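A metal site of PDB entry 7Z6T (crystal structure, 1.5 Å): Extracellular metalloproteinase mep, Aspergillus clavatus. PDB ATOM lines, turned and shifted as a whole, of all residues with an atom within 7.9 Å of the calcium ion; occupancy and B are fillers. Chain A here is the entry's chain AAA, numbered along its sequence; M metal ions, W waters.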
ATOM      1  N   PHE A 113      28.779 -22.838 -14.487  1.00  0.00           N
ATOM      2  CA  PHE A 113      27.618 -22.163 -15.030  1.00  0.00           C
ATOM      3  C   PHE A 113      26.932 -21.397 -13.897  1.00  0.00           C
ATOM      4  O   PHE A 113      26.065 -21.900 -13.192  1.00  0.00           O
ATOM      5  CB  PHE A 113      26.657 -23.173 -15.677  1.00  0.00           C
ATOM      6  CG  PHE A 113      25.516 -22.592 -16.464  1.00  0.00           C
ATOM      7  CD1 PHE A 113      25.732 -21.638 -17.452  1.00  0.00           C
ATOM      8  CD2 PHE A 113      24.206 -23.000 -16.210  1.00  0.00           C
ATOM      9  CE1 PHE A 113      24.687 -21.122 -18.205  1.00  0.00           C
ATOM     10  CE2 PHE A 113      23.156 -22.486 -16.987  1.00  0.00           C
ATOM     11  CZ  PHE A 113      23.399 -21.562 -17.988  1.00  0.00           C
ATOM     12  N   THR A 114      27.328 -20.124 -13.771  1.00  0.00           N
ATOM     13  CA  THR A 114      27.016 -19.304 -12.600  1.00  0.00           C
ATOM     14  C   THR A 114      26.290 -18.054 -13.052  1.00  0.00           C
ATOM     15  O   THR A 114      25.953 -17.918 -14.222  1.00  0.00           O
ATOM     16  CB  THR A 114      28.302 -18.900 -11.883  1.00  0.00           C
ATOM     17  OG1 THR A 114      29.110 -18.116 -12.777  1.00  0.00           O
ATOM     18  CG2 THR A 114      29.081 -20.111 -11.404  1.00  0.00           C
ATOM     19  N   GLU A 115      26.004 -17.133 -12.133  1.00  0.00           N
ATOM     20  CA  GLU A 115      25.234 -15.961 -12.536  1.00  0.00           C
ATOM     21  C   GLU A 115      25.963 -15.211 -13.636  1.00  0.00           C
ATOM     22  O   GLU A 115      25.339 -14.833 -14.656  1.00  0.00           O
ATOM     23  CB  GLU A 115      25.009 -15.002 -11.360  1.00  0.00           C
ATOM     24  CG  GLU A 115      24.443 -15.679 -10.128  1.00  0.00           C
ATOM     25  CD  GLU A 115      25.406 -16.418  -9.211  1.00  0.00           C
ATOM     26  OE1 GLU A 115      26.577 -16.565  -9.518  1.00  0.00           O
ATOM     27  OE2 GLU A 115      24.963 -16.946  -8.211  1.00  0.00           O
ATOM     28  N   LYS A 116      27.285 -15.012 -13.502  1.00  0.00           N
ATOM     29  CA  LYS A 116      27.967 -14.162 -14.483  1.00  0.00           C
ATOM     30  C   LYS A 116      28.163 -14.846 -15.843  1.00  0.00           C
ATOM     31  O   LYS A 116      28.473 -14.171 -16.826  1.00  0.00           O
ATOM     32  CB  LYS A 116      29.315 -13.670 -13.904  1.00  0.00           C
ATOM     33  CG  LYS A 116      30.360 -14.772 -13.679  1.00  0.00           C
ATOM     34  CD  LYS A 116      31.457 -14.311 -12.686  1.00  0.00           C
ATOM     35  CE  LYS A 116      32.233 -13.125 -13.211  1.00  0.00           C
ATOM     36  NZ  LYS A 116      33.042 -12.458 -12.144  1.00  0.00           N
ATOM     37  N   THR A 117      27.957 -16.166 -15.925  1.00  0.00           N
ATOM     38  CA  THR A 117      28.054 -16.859 -17.205  1.00  0.00           C
ATOM     39  C   THR A 117      26.685 -17.114 -17.839  1.00  0.00           C
ATOM     40  O   THR A 117      26.601 -17.733 -18.922  1.00  0.00           O
ATOM     41  CB  THR A 117      28.886 -18.144 -17.120  1.00  0.00           C
ATOM     42  OG1 THR A 117      28.170 -19.072 -16.295  1.00  0.00           O
ATOM     43  CG2 THR A 117      30.277 -17.837 -16.604  1.00  0.00           C
ATOM     44  N   GLY A 118      25.620 -16.602 -17.216  1.00  0.00           N
ATOM     45  CA  GLY A 118      24.319 -16.628 -17.884  1.00  0.00           C
ATOM     46  C   GLY A 118      23.368 -17.728 -17.395  1.00  0.00           C
ATOM     47  O   GLY A 118      22.511 -18.167 -18.168  1.00  0.00           O
ATOM     48  N   ASN A 119      23.433 -18.106 -16.105  1.00  0.00           N
ATOM     49  CA  ASN A 119      22.577 -19.171 -15.592  1.00  0.00           C
ATOM     50  C   ASN A 119      21.166 -18.664 -15.266  1.00  0.00           C
ATOM     51  O   ASN A 119      20.795 -17.544 -15.639  1.00  0.00           O
ATOM     52  CB  ASN A 119      23.232 -19.910 -14.417  1.00  0.00           C
ATOM     53  CG  ASN A 119      23.113 -19.216 -13.077  1.00  0.00           C
ATOM     54  OD1 ASN A 119      22.774 -18.030 -12.973  1.00  0.00           O
ATOM     55  ND2 ASN A 119      23.364 -19.960 -12.007  1.00  0.00           N
ATOM     56  N   PHE A 120      20.347 -19.525 -14.651  1.00  0.00           N
ATOM     57  CA  PHE A 120      18.926 -19.261 -14.444  1.00  0.00           C
ATOM     58  C   PHE A 120      18.631 -19.117 -12.958  1.00  0.00           C
ATOM     59  O   PHE A 120      18.529 -20.110 -12.216  1.00  0.00           O
ATOM     60  CB  PHE A 120      18.114 -20.448 -15.005  1.00  0.00           C
ATOM     61  CG  PHE A 120      18.296 -20.692 -16.479  1.00  0.00           C
ATOM     62  CD1 PHE A 120      17.548 -19.988 -17.418  1.00  0.00           C
ATOM     63  CD2 PHE A 120      19.250 -21.611 -16.954  1.00  0.00           C
ATOM     64  CE1 PHE A 120      17.676 -20.237 -18.776  1.00  0.00           C
ATOM     65  CE2 PHE A 120      19.394 -21.837 -18.322  1.00  0.00           C
ATOM     66  CZ  PHE A 120      18.633 -21.129 -19.241  1.00  0.00           C
ATOM     67  N   GLU A 121      18.466 -17.852 -12.510  1.00  0.00           N
ATOM     68  CA  GLU A 121      18.202 -17.572 -11.110  1.00  0.00           C
ATOM     69  C   GLU A 121      17.399 -16.278 -11.022  1.00  0.00           C
ATOM     70  O   GLU A 121      17.505 -15.400 -11.890  1.00  0.00           O
ATOM     71  CB  GLU A 121      19.482 -17.385 -10.295  1.00  0.00           C
ATOM     72  CG  GLU A 121      20.347 -18.641 -10.299  1.00  0.00           C
ATOM     73  CD  GLU A 121      21.563 -18.428  -9.448  1.00  0.00           C
ATOM     74  OE1 GLU A 121      21.593 -17.335  -8.879  1.00  0.00           O
ATOM     75  OE2 GLU A 121      22.431 -19.317  -9.347  1.00  0.00           O
ATOM     76  N   PHE A 122      16.583 -16.204  -9.954  1.00  0.00           N
ATOM     77  CA  PHE A 122      15.791 -15.024  -9.707  1.00  0.00           C
ATOM     78  C   PHE A 122      16.658 -13.847  -9.222  1.00  0.00           C
ATOM     79  O   PHE A 122      16.598 -12.763  -9.789  1.00  0.00           O
ATOM     80  CB  PHE A 122      14.661 -15.384  -8.737  1.00  0.00           C
ATOM     81  CG  PHE A 122      13.579 -14.347  -8.776  1.00  0.00           C
ATOM     82  CD1 PHE A 122      13.720 -13.213  -8.002  1.00  0.00           C
ATOM     83  CD2 PHE A 122      12.494 -14.481  -9.643  1.00  0.00           C
ATOM     84  CE1 PHE A 122      12.738 -12.220  -8.063  1.00  0.00           C
ATOM     85  CE2 PHE A 122      11.511 -13.498  -9.708  1.00  0.00           C
ATOM     86  CZ  PHE A 122      11.670 -12.370  -8.921  1.00  0.00           C
ATOM     87  N   ASN A 124      20.460 -12.731  -8.411  1.00  0.00           N
ATOM     88  CA  ASN A 124      21.855 -13.057  -8.700  1.00  0.00           C
ATOM     89  C   ASN A 124      22.783 -12.546  -7.591  1.00  0.00           C
ATOM     90  O   ASN A 124      23.986 -12.775  -7.657  1.00  0.00           O
ATOM     91  CB  ASN A 124      22.272 -12.488 -10.063  1.00  0.00           C
ATOM     92  CG  ASN A 124      21.808 -13.312 -11.237  1.00  0.00           C
ATOM     93  OD1 ASN A 124      20.939 -14.193 -11.076  1.00  0.00           O
ATOM     94  ND2 ASN A 124      22.309 -12.963 -12.436  1.00  0.00           N
ATOM     95  N   GLY A 128      26.753 -10.684 -10.952  1.00  0.00           N
ATOM     96  CA  GLY A 128      26.896 -10.457 -12.383  1.00  0.00           C
ATOM     97  C   GLY A 128      25.814 -11.159 -13.194  1.00  0.00           C
ATOM     98  O   GLY A 128      24.991 -11.870 -12.637  1.00  0.00           O
ATOM     99  N   GLY A 129      25.736 -10.808 -14.496  1.00  0.00           N
ATOM    100  CA  GLY A 129      24.655 -11.375 -15.294  1.00  0.00           C
ATOM    101  C   GLY A 129      23.312 -10.722 -14.977  1.00  0.00           C
ATOM    102  O   GLY A 129      23.230  -9.678 -14.301  1.00  0.00           O
ATOM    103  N   ARG A 130      22.241 -11.307 -15.528  1.00  0.00           N
ATOM    104  CA  ARG A 130      20.898 -10.799 -15.337  1.00  0.00           C
ATOM    105  C   ARG A 130      20.083 -11.854 -14.603  1.00  0.00           C
ATOM    106  O   ARG A 130      20.118 -13.053 -14.963  1.00  0.00           O
ATOM    107  CB  ARG A 130      20.284 -10.454 -16.702  1.00  0.00           C
ATOM    108  CG  ARG A 130      21.098  -9.399 -17.437  1.00  0.00           C
ATOM    109  CD  ARG A 130      20.339  -8.866 -18.633  1.00  0.00           C
ATOM    110  NE  ARG A 130      21.240  -8.137 -19.523  1.00  0.00           N
ATOM    111  CZ  ARG A 130      21.703  -6.913 -19.310  1.00  0.00           C
ATOM    112  NH1 ARG A 130      21.344  -6.236 -18.233  1.00  0.00           N
ATOM    113  NH2 ARG A 130      22.529  -6.380 -20.200  1.00  0.00           N
ATOM    114  N   GLY A 131      19.384 -11.424 -13.545  1.00  0.00           N
ATOM    115  CA  GLY A 131      18.486 -12.277 -12.784  1.00  0.00           C
ATOM    116  C   GLY A 131      17.090 -12.289 -13.373  1.00  0.00           C
ATOM    117  O   GLY A 131      16.904 -12.045 -14.588  1.00  0.00           O
ATOM    118  N   ASN A 132      16.123 -12.596 -12.507  1.00  0.00           N
ATOM    119  CA  ASN A 132      14.714 -12.674 -12.828  1.00  0.00           C
ATOM    120  C   ASN A 132      14.433 -13.848 -13.772  1.00  0.00           C
ATOM    121  O   ASN A 132      13.380 -13.906 -14.420  1.00  0.00           O
ATOM    122  CB  ASN A 132      14.201 -11.355 -13.409  1.00  0.00           C
ATOM    123  CG  ASN A 132      12.926 -10.925 -12.738  1.00  0.00           C
ATOM    124  OD1 ASN A 132      12.907  -9.929 -12.008  1.00  0.00           O
ATOM    125  ND2 ASN A 132      11.886 -11.723 -12.897  1.00  0.00           N
ATOM    126  N   ASP A 133      15.373 -14.795 -13.880  1.00  0.00           N
ATOM    127  CA  ASP A 133      15.317 -15.805 -14.927  1.00  0.00           C
ATOM    128  C   ASP A 133      15.515 -17.219 -14.405  1.00  0.00           C
ATOM    129  O   ASP A 133      16.196 -18.041 -15.037  1.00  0.00           O
ATOM    130  CB  ASP A 133      16.228 -15.461 -16.110  1.00  0.00           C
ATOM    131  CG  ASP A 133      17.729 -15.518 -15.855  1.00  0.00           C
ATOM    132  OD1 ASP A 133      18.181 -15.654 -14.688  1.00  0.00           O
ATOM    133  OD2 ASP A 133      18.485 -15.505 -16.854  1.00  0.00           O
ATOM    134  N   TYR A 134      14.918 -17.518 -13.257  1.00  0.00           N
ATOM    135  CA  TYR A 134      14.810 -18.896 -12.834  1.00  0.00           C
ATOM    136  C   TYR A 134      14.059 -19.707 -13.904  1.00  0.00           C
ATOM    137  O   TYR A 134      13.530 -19.161 -14.884  1.00  0.00           O
ATOM    138  CB  TYR A 134      14.189 -19.005 -11.442  1.00  0.00           C
ATOM    139  CG  TYR A 134      12.807 -18.450 -11.223  1.00  0.00           C
ATOM    140  CD1 TYR A 134      12.029 -17.860 -12.219  1.00  0.00           C
ATOM    141  CD2 TYR A 134      12.264 -18.535  -9.944  1.00  0.00           C
ATOM    142  CE1 TYR A 134      10.741 -17.365 -11.953  1.00  0.00           C
ATOM    143  CE2 TYR A 134      10.991 -18.040  -9.652  1.00  0.00           C
ATOM    144  CZ  TYR A 134      10.234 -17.470 -10.661  1.00  0.00           C
ATOM    145  OH  TYR A 134       9.011 -17.017 -10.241  1.00  0.00           O
ATOM    146  N   PRO A 154      17.282 -15.005 -24.083  1.00  0.00           N
ATOM    147  CA  PRO A 154      18.552 -14.441 -23.619  1.00  0.00           C
ATOM    148  C   PRO A 154      18.566 -14.267 -22.097  1.00  0.00           C
ATOM    149  O   PRO A 154      17.525 -14.238 -21.450  1.00  0.00           O
ATOM    150  CB  PRO A 154      18.577 -13.055 -24.300  1.00  0.00           C
ATOM    151  CG  PRO A 154      17.670 -13.200 -25.506  1.00  0.00           C
ATOM    152  CD  PRO A 154      16.600 -14.184 -25.095  1.00  0.00           C
ATOM    153  N   ASP A 155      19.774 -14.080 -21.551  1.00  0.00           N
ATOM    154  CA  ASP A 155      19.930 -13.937 -20.101  1.00  0.00           C
ATOM    155  C   ASP A 155      19.004 -12.828 -19.597  1.00  0.00           C
ATOM    156  O   ASP A 155      18.898 -11.763 -20.215  1.00  0.00           O
ATOM    157  CB  ASP A 155      21.388 -13.599 -19.744  1.00  0.00           C
ATOM    158  CG  ASP A 155      21.727 -13.875 -18.283  1.00  0.00           C
ATOM    159  OD1 ASP A 155      21.006 -14.625 -17.648  1.00  0.00           O
ATOM    160  OD2 ASP A 155      22.736 -13.318 -17.813  1.00  0.00           O
ATOM    161  N   GLY A 156      18.315 -13.103 -18.487  1.00  0.00           N
ATOM    162  CA  GLY A 156      17.422 -12.139 -17.861  1.00  0.00           C
ATOM    163  C   GLY A 156      15.931 -12.373 -18.115  1.00  0.00           C
ATOM    164  O   GLY A 156      15.106 -11.642 -17.573  1.00  0.00           O
ATOM    165  N   GLN A 157      15.584 -13.395 -18.903  1.00  0.00           N
ATOM    166  CA  GLN A 157      14.197 -13.821 -19.012  1.00  0.00           C
ATOM    167  C   GLN A 157      14.159 -15.315 -18.731  1.00  0.00           C
ATOM    168  O   GLN A 157      15.082 -16.026 -19.121  1.00  0.00           O
ATOM    169  CB  GLN A 157      13.634 -13.593 -20.426  1.00  0.00           C
ATOM    170  CG  GLN A 157      13.620 -12.115 -20.825  1.00  0.00           C
ATOM    171  CD  GLN A 157      13.597 -11.964 -22.323  1.00  0.00           C
ATOM    172  OE1 GLN A 157      14.574 -11.576 -22.952  1.00  0.00           O
ATOM    173  NE2 GLN A 157      12.483 -12.322 -22.927  1.00  0.00           N
ATOM    174  N   PRO A 158      13.137 -15.790 -18.002  1.00  0.00           N
ATOM    175  CA  PRO A 158      13.085 -17.165 -17.542  1.00  0.00           C
ATOM    176  C   PRO A 158      13.205 -18.243 -18.600  1.00  0.00           C
ATOM    177  O   PRO A 158      12.611 -18.145 -19.654  1.00  0.00           O
ATOM    178  CB  PRO A 158      11.727 -17.333 -16.826  1.00  0.00           C
ATOM    179  CG  PRO A 158      11.313 -15.912 -16.497  1.00  0.00           C
ATOM    180  CD  PRO A 158      11.938 -15.029 -17.579  1.00  0.00           C
ATOM    181  N   ARG A 193      22.549 -20.743 -23.603  1.00  0.00           N
ATOM    182  CA  ARG A 193      23.096 -19.574 -22.919  1.00  0.00           C
ATOM    183  C   ARG A 193      24.601 -19.450 -23.156  1.00  0.00           C
ATOM    184  O   ARG A 193      25.071 -18.381 -23.539  1.00  0.00           O
ATOM    185  CB  ARG A 193      22.806 -19.627 -21.423  1.00  0.00           C
ATOM    186  CG  ARG A 193      21.352 -19.323 -21.114  1.00  0.00           C
ATOM    187  CD  ARG A 193      21.058 -17.839 -21.134  1.00  0.00           C
ATOM    188  NE  ARG A 193      19.647 -17.522 -20.929  1.00  0.00           N
ATOM    189  CZ  ARG A 193      19.070 -17.283 -19.765  1.00  0.00           C
ATOM    190  NH1 ARG A 193      19.736 -17.464 -18.623  1.00  0.00           N
ATOM    191  NH2 ARG A 193      17.798 -16.903 -19.741  1.00  0.00           N
ATOM    192  N   PRO A 198      25.818 -15.073 -23.221  1.00  0.00           N
ATOM    193  CA  PRO A 198      24.484 -15.115 -22.619  1.00  0.00           C
ATOM    194  C   PRO A 198      23.407 -14.242 -23.257  1.00  0.00           C
ATOM    195  O   PRO A 198      22.220 -14.498 -23.072  1.00  0.00           O
ATOM    196  CB  PRO A 198      24.706 -14.788 -21.134  1.00  0.00           C
ATOM    197  CG  PRO A 198      26.183 -15.023 -20.913  1.00  0.00           C
ATOM    198  CD  PRO A 198      26.856 -14.720 -22.237  1.00  0.00           C
HETATM  199 CA    CA M   1      20.471 -15.250 -15.465  1.00  0.00          CA
HETATM  200  O   HOH W   1      22.779 -14.574 -15.449  1.00  0.00           O
HETATM  201  O   HOH W   2      20.954 -15.781 -13.327  1.00  0.00           O
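Arg 193 touches the calcium ion (NH1 to CA, 3.9 Å).
Of the 25 residues printed, 5 come within 4 Å of the calcium ion.
The nearest printed residue that does not touch the calcium ion is Asn 124 (4.2 Å).
NH1 of Arg 193 lies close to O of Asn 119 (3.2 Å).
The side-chain amide nitrogen (ND2) of Asn 124 sits close to the backbone carbonyl oxygen (O) of Arg 130 (3.3 Å).
The side-chain carboxylate (OD2) of Asp 133 lies close to the backbone NH (N) of Gly 156 (2.9 Å).
The side-chain carboxylate (OD1) of Asp 155 lies close to the guanidinium group (NH1) of Arg 193 (3.3 Å).
N of Asn 119 is in hydrogen-bond range of O of Thr 114, at 3.2 Å.
The side-chain amide oxygen of Asn 119 lies close to the backbone NH of Glu 115, 3.5 Å away.
The side-chain carboxylate (OD2) of Asp 133 lies close to the guanidinium group (NH1) of Arg 193, at 2.9 Å.
NH1 of Arg 193 sits at hydrogen-bond distance from O of Gly 118, 2.9 Å away.
Water W2 lies within hydrogen-bond range of the side-chain amide oxygen of Asn 124 (2.8 Å), the side-chain amide oxygen of Asn 119 (2.9 Å) and the backbone NH of Glu 121 (3.3 Å).
Water W1 lies within hydrogen-bond range of the side-chain carboxylate (OD2) of Asp 155 (2.7 Å), the backbone carbonyl oxygen (O) of Glu 115 (2.7 Å), the backbone NH (N) of Arg 130 (3.3 Å) and the side-chain amide nitrogen (ND2) of Asn 124 (3.4 Å).
Water W2 binds the calcium ion, at 2.3 Å.
The calcium ion is bound by the backbone carbonyl oxygen (O) of Arg 130, at 2.3 Å.
O of Asn 119 binds the calcium ion (2.3 Å).
The calcium ion is bound by the side-chain carboxylate (OD1) of Asp 155, 2.3 Å away.
Water W1 is bound to the calcium ion (2.4 Å).
OD2 of Asp 133 binds the calcium ion.
The calcium ion is bound by OD1 of Asp 133, 2.5 Å away.
The calcium ion has seven donor atoms within binding distance.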
